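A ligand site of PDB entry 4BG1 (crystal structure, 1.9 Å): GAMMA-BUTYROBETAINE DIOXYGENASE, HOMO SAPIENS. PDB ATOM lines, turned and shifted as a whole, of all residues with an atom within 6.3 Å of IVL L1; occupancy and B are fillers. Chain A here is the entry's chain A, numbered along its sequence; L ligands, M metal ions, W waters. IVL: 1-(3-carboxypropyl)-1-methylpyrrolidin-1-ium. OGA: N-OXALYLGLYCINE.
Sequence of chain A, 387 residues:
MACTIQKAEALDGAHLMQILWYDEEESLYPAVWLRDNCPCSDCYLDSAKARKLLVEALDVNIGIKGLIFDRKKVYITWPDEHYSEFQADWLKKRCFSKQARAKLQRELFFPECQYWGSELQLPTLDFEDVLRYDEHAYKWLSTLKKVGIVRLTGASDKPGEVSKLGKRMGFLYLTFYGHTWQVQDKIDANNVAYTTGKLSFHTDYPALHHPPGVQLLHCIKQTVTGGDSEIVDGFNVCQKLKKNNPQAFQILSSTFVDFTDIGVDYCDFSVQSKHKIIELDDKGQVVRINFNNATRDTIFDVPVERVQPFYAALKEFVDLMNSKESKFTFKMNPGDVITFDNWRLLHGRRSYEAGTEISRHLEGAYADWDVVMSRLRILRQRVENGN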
ATOM      1  N   THR A 175       4.386   6.346   0.599  1.00  0.00           N
ATOM      2  CA  THR A 175       3.182   5.942  -0.153  1.00  0.00           C
ATOM      3  C   THR A 175       2.223   5.204   0.791  1.00  0.00           C
ATOM      4  O   THR A 175       2.541   4.988   1.961  1.00  0.00           O
ATOM      5  CB  THR A 175       3.486   5.015  -1.345  1.00  0.00           C
ATOM      6  OG1 THR A 175       3.832   3.688  -0.889  1.00  0.00           O
ATOM      7  CG2 THR A 175       4.602   5.558  -2.190  1.00  0.00           C
ATOM      8  N   TYR A 177       1.687   2.205   1.107  1.00  0.00           N
ATOM      9  CA  TYR A 177       2.263   0.933   1.575  1.00  0.00           C
ATOM     10  C   TYR A 177       3.341   1.129   2.643  1.00  0.00           C
ATOM     11  O   TYR A 177       3.933   0.158   3.101  1.00  0.00           O
ATOM     12  CB  TYR A 177       2.833   0.137   0.386  1.00  0.00           C
ATOM     13  CG  TYR A 177       1.754  -0.443  -0.498  1.00  0.00           C
ATOM     14  CD1 TYR A 177       1.099  -1.639  -0.144  1.00  0.00           C
ATOM     15  CD2 TYR A 177       1.336   0.219  -1.646  1.00  0.00           C
ATOM     16  CE1 TYR A 177       0.101  -2.181  -0.961  1.00  0.00           C
ATOM     17  CE2 TYR A 177       0.326  -0.286  -2.450  1.00  0.00           C
ATOM     18  CZ  TYR A 177      -0.285  -1.498  -2.095  1.00  0.00           C
ATOM     19  OH  TYR A 177      -1.283  -1.995  -2.881  1.00  0.00           O
ATOM     20  N   TRP A 181       8.369  -1.095   3.075  1.00  0.00           N
ATOM     21  CA  TRP A 181       7.375  -2.165   2.993  1.00  0.00           C
ATOM     22  C   TRP A 181       8.047  -3.525   2.895  1.00  0.00           C
ATOM     23  O   TRP A 181       9.194  -3.641   2.414  1.00  0.00           O
ATOM     24  CB  TRP A 181       6.384  -1.945   1.829  1.00  0.00           C
ATOM     25  CG  TRP A 181       6.920  -1.131   0.720  1.00  0.00           C
ATOM     26  CD1 TRP A 181       6.794   0.216   0.565  1.00  0.00           C
ATOM     27  CD2 TRP A 181       7.669  -1.599  -0.415  1.00  0.00           C
ATOM     28  NE1 TRP A 181       7.424   0.620  -0.596  1.00  0.00           N
ATOM     29  CE2 TRP A 181       7.987  -0.462  -1.199  1.00  0.00           C
ATOM     30  CE3 TRP A 181       8.118  -2.853  -0.825  1.00  0.00           C
ATOM     31  CZ2 TRP A 181       8.714  -0.554  -2.384  1.00  0.00           C
ATOM     32  CZ3 TRP A 181       8.837  -2.937  -2.002  1.00  0.00           C
ATOM     33  CH2 TRP A 181       9.123  -1.786  -2.771  1.00  0.00           C
ATOM     34  N   GLN A 182       7.344  -4.562   3.356  1.00  0.00           N
ATOM     35  CA  GLN A 182       7.934  -5.895   3.445  1.00  0.00           C
ATOM     36  C   GLN A 182       7.365  -6.798   2.358  1.00  0.00           C
ATOM     37  O   GLN A 182       6.184  -7.084   2.350  1.00  0.00           O
ATOM     38  CB  GLN A 182       7.753  -6.507   4.840  1.00  0.00           C
ATOM     39  CG  GLN A 182       7.977  -5.535   6.007  1.00  0.00           C
ATOM     40  CD  GLN A 182       9.318  -4.870   5.948  1.00  0.00           C
ATOM     41  OE1 GLN A 182      10.332  -5.498   5.655  1.00  0.00           O
ATOM     42  NE2 GLN A 182       9.349  -3.573   6.255  1.00  0.00           N
ATOM     43  N   VAL A 183       8.222  -7.208   1.412  1.00  0.00           N
ATOM     44  CA  VAL A 183       7.808  -8.132   0.367  1.00  0.00           C
ATOM     45  C   VAL A 183       7.941  -9.556   0.884  1.00  0.00           C
ATOM     46  O   VAL A 183       9.046 -10.069   1.007  1.00  0.00           O
ATOM     47  CB  VAL A 183       8.603  -7.935  -0.949  1.00  0.00           C
ATOM     48  CG1 VAL A 183       8.018  -8.773  -2.067  1.00  0.00           C
ATOM     49  CG2 VAL A 183       8.652  -6.474  -1.339  1.00  0.00           C
ATOM     50  N   ASN A 190      -2.965  -7.788   0.092  1.00  0.00           N
ATOM     51  CA  ASN A 190      -3.513  -6.580  -0.561  1.00  0.00           C
ATOM     52  C   ASN A 190      -2.808  -6.192  -1.862  1.00  0.00           C
ATOM     53  O   ASN A 190      -3.170  -5.172  -2.490  1.00  0.00           O
ATOM     54  CB  ASN A 190      -3.536  -5.395   0.414  1.00  0.00           C
ATOM     55  CG  ASN A 190      -2.133  -4.900   0.806  1.00  0.00           C
ATOM     56  OD1 ASN A 190      -1.107  -5.289   0.229  1.00  0.00           O
ATOM     57  ND2 ASN A 190      -2.103  -4.044   1.821  1.00  0.00           N
ATOM     58  N   ASN A 191      -1.854  -7.005  -2.292  1.00  0.00           N
ATOM     59  CA  ASN A 191      -1.082  -6.747  -3.518  1.00  0.00           C
ATOM     60  C   ASN A 191      -0.517  -8.076  -4.004  1.00  0.00           C
ATOM     61  O   ASN A 191      -0.074  -8.896  -3.190  1.00  0.00           O
ATOM     62  CB  ASN A 191       0.048  -5.746  -3.205  1.00  0.00           C
ATOM     63  CG  ASN A 191       0.677  -5.139  -4.462  1.00  0.00           C
ATOM     64  OD1 ASN A 191       1.449  -5.788  -5.167  1.00  0.00           O
ATOM     65  ND2 ASN A 191       0.365  -3.887  -4.720  1.00  0.00           N
ATOM     66  N   VAL A 192      -0.500  -8.285  -5.320  1.00  0.00           N
ATOM     67  CA  VAL A 192       0.064  -9.532  -5.862  1.00  0.00           C
ATOM     68  C   VAL A 192       1.520  -9.791  -5.457  1.00  0.00           C
ATOM     69  O   VAL A 192       1.944 -10.935  -5.383  1.00  0.00           O
ATOM     70  CB  VAL A 192      -0.065  -9.654  -7.399  1.00  0.00           C
ATOM     71  CG1 VAL A 192      -1.534  -9.655  -7.793  1.00  0.00           C
ATOM     72  CG2 VAL A 192       0.686  -8.548  -8.139  1.00  0.00           C
ATOM     73  N   ALA A 193       2.261  -8.715  -5.181  1.00  0.00           N
ATOM     74  CA  ALA A 193       3.662  -8.848  -4.771  1.00  0.00           C
ATOM     75  C   ALA A 193       3.804  -9.603  -3.459  1.00  0.00           C
ATOM     76  O   ALA A 193       4.828 -10.261  -3.207  1.00  0.00           O
ATOM     77  CB  ALA A 193       4.303  -7.463  -4.668  1.00  0.00           C
ATOM     78  N   TYR A 194       2.764  -9.528  -2.642  1.00  0.00           N
ATOM     79  CA  TYR A 194       2.772 -10.145  -1.323  1.00  0.00           C
ATOM     80  C   TYR A 194       2.208 -11.584  -1.364  1.00  0.00           C
ATOM     81  O   TYR A 194       1.525 -12.030  -0.449  1.00  0.00           O
ATOM     82  CB  TYR A 194       1.995  -9.277  -0.320  1.00  0.00           C
ATOM     83  CG  TYR A 194       2.541  -7.876  -0.086  1.00  0.00           C
ATOM     84  CD1 TYR A 194       3.898  -7.579  -0.246  1.00  0.00           C
ATOM     85  CD2 TYR A 194       1.706  -6.862   0.382  1.00  0.00           C
ATOM     86  CE1 TYR A 194       4.384  -6.308  -0.015  1.00  0.00           C
ATOM     87  CE2 TYR A 194       2.191  -5.581   0.615  1.00  0.00           C
ATOM     88  CZ  TYR A 194       3.533  -5.311   0.427  1.00  0.00           C
ATOM     89  OH  TYR A 194       4.021  -4.072   0.666  1.00  0.00           O
ATOM     90  N   HIS A 202       6.984  -5.345 -14.780  1.00  0.00           N
ATOM     91  CA  HIS A 202       6.167  -4.179 -14.453  1.00  0.00           C
ATOM     92  C   HIS A 202       7.046  -3.041 -13.934  1.00  0.00           C
ATOM     93  O   HIS A 202       8.190  -3.266 -13.517  1.00  0.00           O
ATOM     94  CB  HIS A 202       5.149  -4.530 -13.372  1.00  0.00           C
ATOM     95  CG  HIS A 202       5.773  -4.911 -12.067  1.00  0.00           C
ATOM     96  ND1 HIS A 202       6.397  -6.116 -11.877  1.00  0.00           N
ATOM     97  CD2 HIS A 202       5.896  -4.238 -10.898  1.00  0.00           C
ATOM     98  CE1 HIS A 202       6.857  -6.187 -10.628  1.00  0.00           C
ATOM     99  NE2 HIS A 202       6.553  -5.056 -10.025  1.00  0.00           N
ATOM    100  N   THR A 203       6.494  -1.831 -13.949  1.00  0.00           N
ATOM    101  CA  THR A 203       6.963  -0.685 -13.172  1.00  0.00           C
ATOM    102  C   THR A 203       6.111  -0.639 -11.929  1.00  0.00           C
ATOM    103  O   THR A 203       4.975  -1.056 -11.974  1.00  0.00           O
ATOM    104  CB  THR A 203       6.831   0.642 -13.933  1.00  0.00           C
ATOM    105  OG1 THR A 203       5.461   0.877 -14.320  1.00  0.00           O
ATOM    106  CG2 THR A 203       7.700   0.615 -15.214  1.00  0.00           C
ATOM    107  N   ASP A 204       6.650  -0.130 -10.831  1.00  0.00           N
ATOM    108  CA  ASP A 204       5.849   0.008  -9.608  1.00  0.00           C
ATOM    109  C   ASP A 204       5.010   1.271  -9.590  1.00  0.00           C
ATOM    110  O   ASP A 204       5.459   2.362  -9.942  1.00  0.00           O
ATOM    111  CB  ASP A 204       6.710   0.002  -8.356  1.00  0.00           C
ATOM    112  CG  ASP A 204       6.981  -1.390  -7.819  1.00  0.00           C
ATOM    113  OD1 ASP A 204       6.896  -2.372  -8.583  1.00  0.00           O
ATOM    114  OD2 ASP A 204       7.258  -1.479  -6.592  1.00  0.00           O
ATOM    115  N   TYR A 205       3.761   1.091  -9.171  1.00  0.00           N
ATOM    116  CA  TYR A 205       2.878   2.150  -8.750  1.00  0.00           C
ATOM    117  C   TYR A 205       2.383   3.062  -9.862  1.00  0.00           C
ATOM    118  O   TYR A 205       2.244   4.260  -9.672  1.00  0.00           O
ATOM    119  CB  TYR A 205       3.505   2.967  -7.603  1.00  0.00           C
ATOM    120  CG  TYR A 205       2.676   3.017  -6.313  1.00  0.00           C
ATOM    121  CD1 TYR A 205       1.294   3.151  -6.337  1.00  0.00           C
ATOM    122  CD2 TYR A 205       3.301   2.935  -5.071  1.00  0.00           C
ATOM    123  CE1 TYR A 205       0.558   3.193  -5.163  1.00  0.00           C
ATOM    124  CE2 TYR A 205       2.585   3.000  -3.898  1.00  0.00           C
ATOM    125  CZ  TYR A 205       1.207   3.130  -3.951  1.00  0.00           C
ATOM    126  OH  TYR A 205       0.477   3.184  -2.781  1.00  0.00           O
ATOM    127  N   PRO A 206       2.029   2.495 -11.026  1.00  0.00           N
ATOM    128  CA  PRO A 206       1.393   3.378 -12.014  1.00  0.00           C
ATOM    129  C   PRO A 206       0.011   3.890 -11.600  1.00  0.00           C
ATOM    130  O   PRO A 206      -0.510   4.795 -12.253  1.00  0.00           O
ATOM    131  CB  PRO A 206       1.292   2.522 -13.283  1.00  0.00           C
ATOM    132  CG  PRO A 206       1.322   1.137 -12.768  1.00  0.00           C
ATOM    133  CD  PRO A 206       2.268   1.166 -11.595  1.00  0.00           C
ATOM    134  N   ALA A 207      -0.551   3.338 -10.535  1.00  0.00           N
ATOM    135  CA  ALA A 207      -1.796   3.856  -9.961  1.00  0.00           C
ATOM    136  C   ALA A 207      -1.627   5.285  -9.403  1.00  0.00           C
ATOM    137  O   ALA A 207      -2.621   5.939  -9.125  1.00  0.00           O
ATOM    138  CB  ALA A 207      -2.299   2.922  -8.851  1.00  0.00           C
ATOM    139  N   GLN A 215      13.522   2.956  -7.054  1.00  0.00           N
ATOM    140  CA  GLN A 215      13.093   1.926  -6.144  1.00  0.00           C
ATOM    141  C   GLN A 215      14.327   1.255  -5.482  1.00  0.00           C
ATOM    142  O   GLN A 215      15.352   1.041  -6.118  1.00  0.00           O
ATOM    143  CB  GLN A 215      12.270   0.869  -6.895  1.00  0.00           C
ATOM    144  CG  GLN A 215      11.759  -0.272  -6.045  1.00  0.00           C
ATOM    145  CD  GLN A 215      10.648  -1.090  -6.719  1.00  0.00           C
ATOM    146  OE1 GLN A 215      10.360  -2.212  -6.321  1.00  0.00           O
ATOM    147  NE2 GLN A 215      10.055  -0.543  -7.748  1.00  0.00           N
ATOM    148  N   ASP A 261      -5.931   0.954  -7.449  1.00  0.00           N
ATOM    149  CA  ASP A 261      -5.465   0.212  -6.283  1.00  0.00           C
ATOM    150  C   ASP A 261      -6.362   0.606  -5.113  1.00  0.00           C
ATOM    151  O   ASP A 261      -6.420   1.789  -4.743  1.00  0.00           O
ATOM    152  CB  ASP A 261      -4.020   0.572  -5.965  1.00  0.00           C
ATOM    153  CG  ASP A 261      -3.310  -0.447  -5.077  1.00  0.00           C
ATOM    154  OD1 ASP A 261      -3.764  -1.622  -4.989  1.00  0.00           O
ATOM    155  OD2 ASP A 261      -2.273  -0.054  -4.475  1.00  0.00           O
ATOM    156  N   ASN A 292       1.933  -1.755 -14.918  1.00  0.00           N
ATOM    157  CA  ASN A 292       1.838  -2.899 -14.020  1.00  0.00           C
ATOM    158  C   ASN A 292       0.538  -3.637 -14.363  1.00  0.00           C
ATOM    159  O   ASN A 292      -0.526  -3.094 -14.194  1.00  0.00           O
ATOM    160  CB  ASN A 292       1.791  -2.463 -12.567  1.00  0.00           C
ATOM    161  CG  ASN A 292       1.778  -3.639 -11.609  1.00  0.00           C
ATOM    162  OD1 ASN A 292       1.604  -4.800 -12.019  1.00  0.00           O
ATOM    163  ND2 ASN A 292       1.951  -3.374 -10.314  1.00  0.00           N
ATOM    164  N   THR A 295      -2.357  -3.984 -11.620  1.00  0.00           N
ATOM    165  CA  THR A 295      -3.126  -2.817 -11.216  1.00  0.00           C
ATOM    166  C   THR A 295      -3.764  -2.086 -12.372  1.00  0.00           C
ATOM    167  O   THR A 295      -4.472  -1.100 -12.165  1.00  0.00           O
ATOM    168  CB  THR A 295      -2.255  -1.829 -10.395  1.00  0.00           C
ATOM    169  OG1 THR A 295      -1.176  -1.328 -11.201  1.00  0.00           O
ATOM    170  CG2 THR A 295      -1.698  -2.515  -9.194  1.00  0.00           C
ATOM    171  N   TYR A 366      10.986   3.721  -1.856  1.00  0.00           N
ATOM    172  CA  TYR A 366      11.051   4.548  -3.046  1.00  0.00           C
ATOM    173  C   TYR A 366      11.719   5.894  -2.723  1.00  0.00           C
ATOM    174  O   TYR A 366      11.708   6.330  -1.572  1.00  0.00           O
ATOM    175  CB  TYR A 366       9.633   4.855  -3.568  1.00  0.00           C
ATOM    176  CG  TYR A 366       8.792   3.650  -3.930  1.00  0.00           C
ATOM    177  CD1 TYR A 366       9.185   2.793  -4.955  1.00  0.00           C
ATOM    178  CD2 TYR A 366       7.568   3.403  -3.305  1.00  0.00           C
ATOM    179  CE1 TYR A 366       8.427   1.688  -5.310  1.00  0.00           C
ATOM    180  CE2 TYR A 366       6.795   2.294  -3.648  1.00  0.00           C
ATOM    181  CZ  TYR A 366       7.222   1.451  -4.673  1.00  0.00           C
ATOM    182  OH  TYR A 366       6.489   0.334  -5.051  1.00  0.00           O
HETATM  183  CAF IVL L   1       5.698  -3.062  -3.116  1.00  0.00           C
HETATM  184  CAE IVL L   1       5.191  -4.442  -2.784  1.00  0.00           C
HETATM  185  CAD IVL L   1       3.692  -4.429  -2.997  1.00  0.00           C
HETATM  186  CAA IVL L   1       3.324  -2.967  -2.827  1.00  0.00           C
HETATM  187  CAH IVL L   1       4.636  -0.872  -2.775  1.00  0.00           C
HETATM  188  CAJ IVL L   1       4.585  -2.198  -4.829  1.00  0.00           C
HETATM  189  CAK IVL L   1       3.501  -1.553  -5.590  1.00  0.00           C
HETATM  190  CAL IVL L   1       3.493  -2.299  -6.951  1.00  0.00           C
HETATM  191  CAM IVL L   1       2.239  -1.784  -7.560  1.00  0.00           C
HETATM  192  N3  IVL L   1       4.493  -2.219  -3.371  1.00  0.00           N
HETATM  193  OAB IVL L   1       2.215  -1.188  -8.609  1.00  0.00           O
HETATM  194  OAC IVL L   1       1.157  -1.969  -6.850  1.00  0.00           O
HETATM  195  C1  OGA L   2       7.386  -5.697  -5.926  1.00  0.00           C
HETATM  196  C2  OGA L   2       8.379  -6.483  -6.644  1.00  0.00           C
HETATM  197  C4  OGA L   2      10.161  -8.109  -6.612  1.00  0.00           C
HETATM  198  C5  OGA L   2      10.506  -9.374  -5.838  1.00  0.00           C
HETATM  199  O1  OGA L   2       7.193  -5.950  -4.706  1.00  0.00           O
HETATM  200  O2  OGA L   2       6.791  -4.785  -6.556  1.00  0.00           O
HETATM  201  O2' OGA L   2       8.632  -6.183  -7.805  1.00  0.00           O
HETATM  202  O3  OGA L   2      11.521 -10.000  -6.196  1.00  0.00           O
HETATM  203  N1  OGA L   2       9.006  -7.444  -6.006  1.00  0.00           N
HETATM  204  O4  OGA L   2       9.785  -9.737  -4.896  1.00  0.00           O
HETATM  205 ZN    ZN M   1       7.633  -4.329  -8.351  1.00  0.00          ZN
HETATM  206  O   HOH W   1      -0.101   0.551  -9.230  1.00  0.00           O
HETATM  207  O   HOH W   2       1.336  -5.125  -7.872  1.00  0.00           O
HETATM  208  O   HOH W   3      -0.586  -0.054  -6.654  1.00  0.00           O
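CD2 of Tyr 177 touches CAH of IVL L1, 3.7 Å away.
Trp 181 touches IVL L1.
Ala 193 touches IVL L1.
Tyr 194 touches IVL L1 (CE1 to CAE, 3.4 Å).
Asp 204 touches IVL L1 (OD2 to CAJ, 3.3 Å).
CD of Pro 206 touches OAB of IVL L1, at 3.8 Å.
Thr 295 touches IVL L1.
Tyr 366 touches IVL L1 (OH to CAH, 3.2 Å).
Hydrophobic or aromatic side chains within 4 Å of IVL L1: Tyr 177, Trp 181, Ala 193, Tyr 194, Pro 206 and Tyr 366.
Of the 21 residues printed, 11 come within 4 Å of IVL L1.
The nearest printed residue that does not touch IVL L1 is Val 183 (4.3 Å).
An oxygen (OAB) of IVL L1 sits at hydrogen-bond distance from the side-chain amide nitrogen of Asn 292, 2.8 Å away.
N of Tyr 205 sits at hydrogen-bond distance from OAB of IVL L1.
OAC of IVL L1 sits at hydrogen-bond distance from ND2 of Asn 191 (3.0 Å).
Water W3 bridges OAC of IVL L1 and OD2 of Asp 261.
Water W1 lies within hydrogen-bond range of OG1 of Thr 295 (2.9 Å), OAB of IVL L1 (3.0 Å) and N of Ala 207 (3.1 Å).
Water W2 lies within hydrogen-bond range of OD1 of Asn 191 (2.8 Å), ND2 of Asn 292 (3.1 Å) and OAC of IVL L1 (3.3 Å).
The side-chain amide oxygen (OD1) of Asn 191 lies within hydrogen-bond range of the backbone NH (N) of Ala 193 (3.0 Å).
The side-chain amide nitrogen (ND2) of Asn 191 sits at hydrogen-bond distance from the side-chain hydroxyl (OH) of Tyr 177 (3.1 Å).
The side-chain carboxylate (OD2) of Asp 204 lies within hydrogen-bond range of the side-chain hydroxyl (OH) of Tyr 366 (2.5 Å).
The side-chain carboxylate (OD2) of Asp 204 is in hydrogen-bond range of the side-chain amide nitrogen (NE2) of Gln 215 (3.2 Å).
The side-chain hydroxyl (OH) of Tyr 177 lies within hydrogen-bond range of the side-chain carboxylate (OD2) of Asp 261 (2.7 Å).
N of Tyr 177 sits close to OG1 of Thr 175, at 3.3 Å.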
